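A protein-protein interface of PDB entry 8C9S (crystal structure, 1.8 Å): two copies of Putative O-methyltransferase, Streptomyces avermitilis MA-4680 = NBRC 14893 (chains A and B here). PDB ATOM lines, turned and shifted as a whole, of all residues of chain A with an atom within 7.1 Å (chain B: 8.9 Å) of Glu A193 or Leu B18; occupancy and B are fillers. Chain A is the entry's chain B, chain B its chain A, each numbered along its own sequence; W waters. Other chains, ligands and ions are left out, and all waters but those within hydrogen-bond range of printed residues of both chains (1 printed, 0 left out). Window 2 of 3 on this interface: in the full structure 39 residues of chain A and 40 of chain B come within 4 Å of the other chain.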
ATOM      1  N   VAL A 175      16.497   8.498  30.077  1.00  0.00           N
ATOM      2  CA  VAL A 175      16.369   7.513  28.964  1.00  0.00           C
ATOM      3  C   VAL A 175      16.525   6.085  29.491  1.00  0.00           C
ATOM      4  O   VAL A 175      16.021   5.171  28.832  1.00  0.00           O
ATOM      5  CB  VAL A 175      17.334   7.801  27.790  1.00  0.00           C
ATOM      6  CG1 VAL A 175      18.795   7.611  28.164  1.00  0.00           C
ATOM      7  CG2 VAL A 175      16.991   6.960  26.584  1.00  0.00           C
ATOM      8  N   ARG A 186       9.957   7.817  26.395  1.00  0.00           N
ATOM      9  CA  ARG A 186       9.345   6.595  25.822  1.00  0.00           C
ATOM     10  C   ARG A 186       9.614   6.567  24.314  1.00  0.00           C
ATOM     11  O   ARG A 186       9.988   5.485  23.801  1.00  0.00           O
ATOM     12  CB  ARG A 186       7.869   6.498  26.223  1.00  0.00           C
ATOM     13  CG  ARG A 186       7.721   6.097  27.690  1.00  0.00           C
ATOM     14  CD  ARG A 186       6.298   5.802  28.093  1.00  0.00           C
ATOM     15  NE  ARG A 186       5.241   6.666  27.535  1.00  0.00           N
ATOM     16  CZ  ARG A 186       4.359   7.367  28.263  1.00  0.00           C
ATOM     17  NH1 ARG A 186       3.411   8.076  27.660  1.00  0.00           N
ATOM     18  NH2 ARG A 186       4.413   7.333  29.592  1.00  0.00           N
ATOM     19  N   GLY A 187       9.494   7.705  23.654  1.00  0.00           N
ATOM     20  CA  GLY A 187       9.759   7.804  22.212  1.00  0.00           C
ATOM     21  C   GLY A 187      11.225   7.597  21.941  1.00  0.00           C
ATOM     22  O   GLY A 187      11.577   6.957  20.921  1.00  0.00           O
ATOM     23  N   THR A 188      12.077   8.159  22.779  1.00  0.00           N
ATOM     24  CA  THR A 188      13.542   7.985  22.620  1.00  0.00           C
ATOM     25  C   THR A 188      13.883   6.496  22.782  1.00  0.00           C
ATOM     26  O   THR A 188      14.529   5.930  21.882  1.00  0.00           O
ATOM     27  CB  THR A 188      14.347   8.862  23.577  1.00  0.00           C
ATOM     28  OG1 THR A 188      14.027  10.214  23.281  1.00  0.00           O
ATOM     29  CG2 THR A 188      15.837   8.639  23.445  1.00  0.00           C
ATOM     30  N   ARG A 189      13.462   5.846  23.868  1.00  0.00           N
ATOM     31  CA  ARG A 189      13.752   4.407  24.063  1.00  0.00           C
ATOM     32  C   ARG A 189      13.230   3.596  22.879  1.00  0.00           C
ATOM     33  O   ARG A 189      13.959   2.708  22.444  1.00  0.00           O
ATOM     34  CB  ARG A 189      13.164   3.859  25.374  1.00  0.00           C
ATOM     35  CG  ARG A 189      13.772   4.482  26.623  1.00  0.00           C
ATOM     36  CD  ARG A 189      13.071   4.034  27.892  1.00  0.00           C
ATOM     37  NE  ARG A 189      13.093   2.581  27.992  1.00  0.00           N
ATOM     38  CZ  ARG A 189      14.120   1.852  28.472  1.00  0.00           C
ATOM     39  NH1 ARG A 189      15.205   2.416  28.951  1.00  0.00           N
ATOM     40  NH2 ARG A 189      14.017   0.546  28.531  1.00  0.00           N
ATOM     41  N   SER A 190      12.012   3.847  22.393  1.00  0.00           N
ATOM     42  CA  SER A 190      11.416   3.060  21.284  1.00  0.00           C
ATOM     43  C   SER A 190      12.249   3.237  20.010  1.00  0.00           C
ATOM     44  O   SER A 190      12.444   2.251  19.302  1.00  0.00           O
ATOM     45  CB  SER A 190       9.951   3.404  21.054  1.00  0.00           C
ATOM     46  OG  SER A 190       9.177   3.012  22.184  1.00  0.00           O
ATOM     47  N   ALA A 191      12.671   4.461  19.685  1.00  0.00           N
ATOM     48  CA  ALA A 191      13.488   4.717  18.477  1.00  0.00           C
ATOM     49  C   ALA A 191      14.849   4.025  18.613  1.00  0.00           C
ATOM     50  O   ALA A 191      15.319   3.442  17.633  1.00  0.00           O
ATOM     51  CB  ALA A 191      13.618   6.183  18.246  1.00  0.00           C
ATOM     52  N   LEU A 192      15.483   4.056  19.788  1.00  0.00           N
ATOM     53  CA  LEU A 192      16.795   3.387  19.936  1.00  0.00           C
ATOM     54  C   LEU A 192      16.644   1.859  19.788  1.00  0.00           C
ATOM     55  O   LEU A 192      17.516   1.221  19.208  1.00  0.00           O
ATOM     56  CB  LEU A 192      17.391   3.783  21.275  1.00  0.00           C
ATOM     57  CG  LEU A 192      17.747   5.256  21.403  1.00  0.00           C
ATOM     58  CD1 LEU A 192      18.343   5.512  22.761  1.00  0.00           C
ATOM     59  CD2 LEU A 192      18.700   5.701  20.303  1.00  0.00           C
ATOM     60  N   GLU A 193      15.596   1.278  20.350  1.00  0.00           N
ATOM     61  CA  GLU A 193      15.332  -0.182  20.242  1.00  0.00           C
ATOM     62  C   GLU A 193      15.030  -0.528  18.781  1.00  0.00           C
ATOM     63  O   GLU A 193      15.473  -1.607  18.320  1.00  0.00           O
ATOM     64  CB  GLU A 193      14.243  -0.590  21.242  1.00  0.00           C
ATOM     65  CG  GLU A 193      14.833  -0.714  22.637  1.00  0.00           C
ATOM     66  CD  GLU A 193      13.943  -0.383  23.819  1.00  0.00           C
ATOM     67  OE1 GLU A 193      12.719  -0.476  23.632  1.00  0.00           O
ATOM     68  OE2 GLU A 193      14.497  -0.015  24.924  1.00  0.00           O
ATOM     69  N   LEU A 194      14.356   0.369  18.051  1.00  0.00           N
ATOM     70  CA  LEU A 194      14.023   0.127  16.623  1.00  0.00           C
ATOM     71  C   LEU A 194      15.325   0.123  15.809  1.00  0.00           C
ATOM     72  O   LEU A 194      15.500  -0.751  14.982  1.00  0.00           O
ATOM     73  CB  LEU A 194      13.036   1.193  16.140  1.00  0.00           C
ATOM     74  CG  LEU A 194      12.708   1.143  14.650  1.00  0.00           C
ATOM     75  CD1 LEU A 194      12.111  -0.205  14.267  1.00  0.00           C
ATOM     76  CD2 LEU A 194      11.753   2.258  14.278  1.00  0.00           C
ATOM     77  N   ILE A 195      16.244   1.048  16.082  1.00  0.00           N
ATOM     78  CA  ILE A 195      17.586   1.045  15.446  1.00  0.00           C
ATOM     79  C   ILE A 195      18.296  -0.283  15.761  1.00  0.00           C
ATOM     80  O   ILE A 195      18.828  -0.886  14.841  1.00  0.00           O
ATOM     81  CB  ILE A 195      18.431   2.260  15.874  1.00  0.00           C
ATOM     82  CG1 ILE A 195      17.790   3.560  15.382  1.00  0.00           C
ATOM     83  CG2 ILE A 195      19.846   2.100  15.353  1.00  0.00           C
ATOM     84  CD1 ILE A 195      18.325   4.805  16.044  1.00  0.00           C
ATOM     85  N   ALA A 196      18.282  -0.748  17.014  1.00  0.00           N
ATOM     86  CA  ALA A 196      18.985  -1.979  17.421  1.00  0.00           C
ATOM     87  C   ALA A 196      18.380  -3.178  16.680  1.00  0.00           C
ATOM     88  O   ALA A 196      19.140  -3.889  15.981  1.00  0.00           O
ATOM     89  CB  ALA A 196      18.897  -2.153  18.919  1.00  0.00           C
ATOM     90  N   GLU A 197      17.057  -3.335  16.733  1.00  0.00           N
ATOM     91  CA  GLU A 197      16.372  -4.559  16.249  1.00  0.00           C
ATOM     92  C   GLU A 197      16.292  -4.606  14.726  1.00  0.00           C
ATOM     93  O   GLU A 197      16.245  -5.724  14.213  1.00  0.00           O
ATOM     94  CB  GLU A 197      14.963  -4.691  16.817  1.00  0.00           C
ATOM     95  CG  GLU A 197      14.965  -4.890  18.323  1.00  0.00           C
ATOM     96  CD  GLU A 197      13.633  -5.303  18.947  1.00  0.00           C
ATOM     97  OE1 GLU A 197      12.865  -6.025  18.292  1.00  0.00           O
ATOM     98  OE2 GLU A 197      13.371  -4.899  20.083  1.00  0.00           O
ATOM     99  N   HIS A 198      16.196  -3.473  14.032  1.00  0.00           N
ATOM    100  CA  HIS A 198      15.930  -3.467  12.576  1.00  0.00           C
ATOM    101  C   HIS A 198      17.166  -3.969  11.835  1.00  0.00           C
ATOM    102  O   HIS A 198      18.269  -3.474  12.029  1.00  0.00           O
ATOM    103  CB  HIS A 198      15.478  -2.081  12.094  1.00  0.00           C
ATOM    104  CG  HIS A 198      14.576  -2.169  10.913  1.00  0.00           C
ATOM    105  ND1 HIS A 198      15.025  -2.587   9.674  1.00  0.00           N
ATOM    106  CD2 HIS A 198      13.249  -2.006  10.794  1.00  0.00           C
ATOM    107  CE1 HIS A 198      14.017  -2.611   8.822  1.00  0.00           C
ATOM    108  NE2 HIS A 198      12.930  -2.278   9.490  1.00  0.00           N
ATOM    109  N   GLY A 203      23.624   1.519  14.501  1.00  0.00           N
ATOM    110  CA  GLY A 203      23.868   2.844  15.083  1.00  0.00           C
ATOM    111  C   GLY A 203      24.702   2.846  16.333  1.00  0.00           C
ATOM    112  O   GLY A 203      25.218   1.796  16.761  1.00  0.00           O
ATOM    113  N   VAL B  11      23.668   5.499  31.630  1.00  0.00           N
ATOM    114  CA  VAL B  11      23.250   5.875  30.247  1.00  0.00           C
ATOM    115  C   VAL B  11      24.144   5.145  29.229  1.00  0.00           C
ATOM    116  O   VAL B  11      23.614   4.557  28.270  1.00  0.00           O
ATOM    117  CB  VAL B  11      23.258   7.399  30.055  1.00  0.00           C
ATOM    118  CG1 VAL B  11      23.016   7.772  28.603  1.00  0.00           C
ATOM    119  CG2 VAL B  11      22.236   8.077  30.941  1.00  0.00           C
ATOM    120  N   ASP B  12      25.462   5.124  29.424  1.00  0.00           N
ATOM    121  CA  ASP B  12      26.375   4.411  28.494  1.00  0.00           C
ATOM    122  C   ASP B  12      26.105   2.911  28.511  1.00  0.00           C
ATOM    123  O   ASP B  12      26.179   2.295  27.428  1.00  0.00           O
ATOM    124  CB  ASP B  12      27.856   4.625  28.804  1.00  0.00           C
ATOM    125  CG  ASP B  12      28.503   5.609  27.836  1.00  0.00           C
ATOM    126  OD1 ASP B  12      27.750   6.313  27.123  1.00  0.00           O
ATOM    127  OD2 ASP B  12      29.755   5.711  27.847  1.00  0.00           O
ATOM    128  N   ASP B  13      25.856   2.324  29.682  1.00  0.00           N
ATOM    129  CA  ASP B  13      25.522   0.874  29.756  1.00  0.00           C
ATOM    130  C   ASP B  13      24.292   0.579  28.885  1.00  0.00           C
ATOM    131  O   ASP B  13      24.311  -0.419  28.140  1.00  0.00           O
ATOM    132  CB  ASP B  13      25.282   0.399  31.180  1.00  0.00           C
ATOM    133  CG  ASP B  13      25.127  -1.113  31.238  1.00  0.00           C
ATOM    134  OD1 ASP B  13      26.026  -1.824  30.734  1.00  0.00           O
ATOM    135  OD2 ASP B  13      24.102  -1.564  31.749  1.00  0.00           O
ATOM    136  N   TYR B  14      23.251   1.401  28.975  1.00  0.00           N
ATOM    137  CA  TYR B  14      22.017   1.240  28.166  1.00  0.00           C
ATOM    138  C   TYR B  14      22.370   1.342  26.686  1.00  0.00           C
ATOM    139  O   TYR B  14      21.996   0.450  25.922  1.00  0.00           O
ATOM    140  CB  TYR B  14      20.996   2.291  28.565  1.00  0.00           C
ATOM    141  CG  TYR B  14      19.761   2.330  27.712  1.00  0.00           C
ATOM    142  CD1 TYR B  14      18.898   1.254  27.669  1.00  0.00           C
ATOM    143  CD2 TYR B  14      19.466   3.439  26.931  1.00  0.00           C
ATOM    144  CE1 TYR B  14      17.748   1.289  26.896  1.00  0.00           C
ATOM    145  CE2 TYR B  14      18.317   3.487  26.149  1.00  0.00           C
ATOM    146  CZ  TYR B  14      17.464   2.405  26.120  1.00  0.00           C
ATOM    147  OH  TYR B  14      16.326   2.427  25.358  1.00  0.00           O
ATOM    148  N   PHE B  15      23.083   2.407  26.284  1.00  0.00           N
ATOM    149  CA  PHE B  15      23.418   2.679  24.856  1.00  0.00           C
ATOM    150  C   PHE B  15      24.298   1.576  24.288  1.00  0.00           C
ATOM    151  O   PHE B  15      24.061   1.140  23.147  1.00  0.00           O
ATOM    152  CB  PHE B  15      24.160   4.011  24.699  1.00  0.00           C
ATOM    153  CG  PHE B  15      23.331   5.258  24.864  1.00  0.00           C
ATOM    154  CD1 PHE B  15      21.945   5.213  24.883  1.00  0.00           C
ATOM    155  CD2 PHE B  15      23.956   6.509  24.937  1.00  0.00           C
ATOM    156  CE1 PHE B  15      21.198   6.375  25.009  1.00  0.00           C
ATOM    157  CE2 PHE B  15      23.202   7.662  25.024  1.00  0.00           C
ATOM    158  CZ  PHE B  15      21.824   7.592  25.079  1.00  0.00           C
ATOM    159  N   THR B  16      25.324   1.159  25.030  1.00  0.00           N
ATOM    160  CA  THR B  16      26.276   0.119  24.568  1.00  0.00           C
ATOM    161  C   THR B  16      25.568  -1.230  24.424  1.00  0.00           C
ATOM    162  O   THR B  16      25.692  -1.857  23.387  1.00  0.00           O
ATOM    163  CB  THR B  16      27.490   0.019  25.496  1.00  0.00           C
ATOM    164  OG1 THR B  16      28.139   1.271  25.261  1.00  0.00           O
ATOM    165  CG2 THR B  16      28.385  -1.153  25.164  1.00  0.00           C
ATOM    166  N   THR B  17      24.861  -1.695  25.445  1.00  0.00           N
ATOM    167  CA  THR B  17      24.251  -3.049  25.376  1.00  0.00           C
ATOM    168  C   THR B  17      23.204  -3.054  24.244  1.00  0.00           C
ATOM    169  O   THR B  17      23.077  -4.078  23.547  1.00  0.00           O
ATOM    170  CB  THR B  17      23.803  -3.490  26.770  1.00  0.00           C
ATOM    171  OG1 THR B  17      22.758  -2.629  27.187  1.00  0.00           O
ATOM    172  CG2 THR B  17      24.920  -3.423  27.779  1.00  0.00           C
ATOM    173  N   LEU B  18      22.547  -1.928  23.973  1.00  0.00           N
ATOM    174  CA  LEU B  18      21.486  -1.848  22.946  1.00  0.00           C
ATOM    175  C   LEU B  18      22.105  -1.696  21.551  1.00  0.00           C
ATOM    176  O   LEU B  18      21.755  -2.465  20.654  1.00  0.00           O
ATOM    177  CB  LEU B  18      20.564  -0.684  23.313  1.00  0.00           C
ATOM    178  CG  LEU B  18      19.307  -0.551  22.475  1.00  0.00           C
ATOM    179  CD1 LEU B  18      18.518  -1.845  22.491  1.00  0.00           C
ATOM    180  CD2 LEU B  18      18.444   0.607  22.980  1.00  0.00           C
ATOM    181  N   LEU B  19      23.001  -0.747  21.358  1.00  0.00           N
ATOM    182  CA  LEU B  19      23.436  -0.316  19.997  1.00  0.00           C
ATOM    183  C   LEU B  19      24.835  -0.815  19.634  1.00  0.00           C
ATOM    184  O   LEU B  19      25.085  -0.944  18.424  1.00  0.00           O
ATOM    185  CB  LEU B  19      23.414   1.216  19.955  1.00  0.00           C
ATOM    186  CG  LEU B  19      22.031   1.819  20.166  1.00  0.00           C
ATOM    187  CD1 LEU B  19      22.115   3.323  20.288  1.00  0.00           C
ATOM    188  CD2 LEU B  19      21.091   1.403  19.061  1.00  0.00           C
ATOM    189  N   ALA B  20      25.736  -0.970  20.608  1.00  0.00           N
ATOM    190  CA  ALA B  20      27.166  -1.249  20.353  1.00  0.00           C
ATOM    191  C   ALA B  20      27.630  -2.422  21.208  1.00  0.00           C
ATOM    192  O   ALA B  20      28.633  -2.309  21.913  1.00  0.00           O
ATOM    193  CB  ALA B  20      27.998  -0.009  20.617  1.00  0.00           C
ATOM    194  N   PRO B  21      26.926  -3.568  21.184  1.00  0.00           N
ATOM    195  CA  PRO B  21      27.317  -4.709  21.999  1.00  0.00           C
ATOM    196  C   PRO B  21      28.698  -5.243  21.584  1.00  0.00           C
ATOM    197  O   PRO B  21      29.031  -5.247  20.419  1.00  0.00           O
ATOM    198  CB  PRO B  21      26.213  -5.739  21.750  1.00  0.00           C
ATOM    199  CG  PRO B  21      25.638  -5.364  20.424  1.00  0.00           C
ATOM    200  CD  PRO B  21      25.749  -3.856  20.352  1.00  0.00           C
ATOM    201  N   GLU B  22      29.488  -5.619  22.580  1.00  0.00           N
ATOM    202  CA  GLU B  22      30.854  -6.156  22.404  1.00  0.00           C
ATOM    203  C   GLU B  22      30.709  -7.667  22.239  1.00  0.00           C
ATOM    204  O   GLU B  22      30.115  -8.264  23.119  1.00  0.00           O
ATOM    205  CB  GLU B  22      31.714  -5.829  23.623  1.00  0.00           C
ATOM    206  CG  GLU B  22      32.081  -4.363  23.740  1.00  0.00           C
ATOM    207  CD  GLU B  22      32.727  -4.005  25.066  1.00  0.00           C
ATOM    208  OE1 GLU B  22      32.127  -4.307  26.108  1.00  0.00           O
ATOM    209  OE2 GLU B  22      33.804  -3.422  25.058  1.00  0.00           O
ATOM    210  N   LYS B  49      32.106   2.078  18.010  1.00  0.00           N
ATOM    211  CA  LYS B  49      31.012   1.928  17.031  1.00  0.00           C
ATOM    212  C   LYS B  49      30.956   3.224  16.203  1.00  0.00           C
ATOM    213  O   LYS B  49      30.847   3.129  14.959  1.00  0.00           O
ATOM    214  CB  LYS B  49      29.717   1.588  17.748  1.00  0.00           C
ATOM    215  CG  LYS B  49      28.533   1.321  16.827  1.00  0.00           C
ATOM    216  CD  LYS B  49      28.660   0.023  16.057  1.00  0.00           C
ATOM    217  CE  LYS B  49      27.609  -0.240  15.003  1.00  0.00           C
ATOM    218  NZ  LYS B  49      26.267  -0.479  15.569  1.00  0.00           N
HETATM  219  O   HOH W   1      23.034  -0.670  16.359  1.00  0.00           O
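Among the printed residues, pairs that only touch across the chains: Val A175 with Tyr B14, Arg A189 with Tyr B14, Leu A192 with Tyr B14, Leu A192 with Phe B15, Leu A192 with Leu B18, Leu A192 with Leu B19, Glu A193 with Leu B18, Ile A195 with Leu B19 and Ala A196 with Leu B18.
The guanidinium group of Arg A189 is in hydrogen-bond range of the backbone carbonyl oxygen of Val A175 (2.9 Å). The guanidinium group of Arg A189 is in salt-bridge range of the side-chain carboxylate of Glu A193, at 3.7 Å. O of Leu B19 sits at hydrogen-bond distance from NZ of Lys B49 (3.1 Å). OG1 of Thr B17 sits at hydrogen-bond distance from O of Tyr B14 (3.4 Å).
Water W1 lies within hydrogen-bond range of the backbone carbonyl oxygen (O) of Leu B19 (2.9 Å), the backbone NH (N) of Gly A203 (2.9 Å) and the side-chain amino group (NZ) of Lys B49 (3.3 Å).
Thr A188 touches none of the printed residues of chain B. Of the printed residues of chain B, Arg A189 touches Tyr B14 (3.5 Å). Glu A193 touches just these residues of chain B: Tyr B14 (3.1 Å) and Leu B18 (3.9 Å). Of the printed residues of chain B, Ile A195 touches Leu B19. Leu B18 touches just these residues of chain A: Leu A192, Glu A193 and Ala A196. Of the printed residues of chain A, Leu B19 touches Leu A192, Ile A195 and Gly A203. Printed residues of chain A within 4 Å of Lys B49: Gly A203 (2.8 Å). The nearest residue of chain B that does not touch Glu A193 is Leu B19 (5.6 Å).
No position is printed for both chains. Of the 12 pairs that touch across the chains among the printed residues, none has its exchanged pair printed and touching as well.
Along chain A the printed residues that touch a printed residue of chain B span positions 175 to 203. Of the 13 printed residues of chain B, 5 touch a printed residue of chain A. Printed residues of chain B that touch a printed residue of chain A: Tyr B14, Phe B15, Leu B18, Leu B19 and Lys B49. Hydrophobic or aromatic side chains of chain B that line the printed part of chain A: Tyr B14, Phe B15, Leu B18 and Leu B19. Among the printed residues, no Asp or Glu carboxylate lies within 4 Å of a Lys or Arg side-chain nitrogen of the other chain.
The side-chain amino group (NZ) of Lys B49 lies within hydrogen-bond range of the backbone carbonyl oxygen (O) of Gly A203 (2.8 Å). O of Gly A203 lies close to O of Leu B19, at 3.2 Å. OH of Tyr B14 is in hydrogen-bond range of OE2 of Glu A193.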
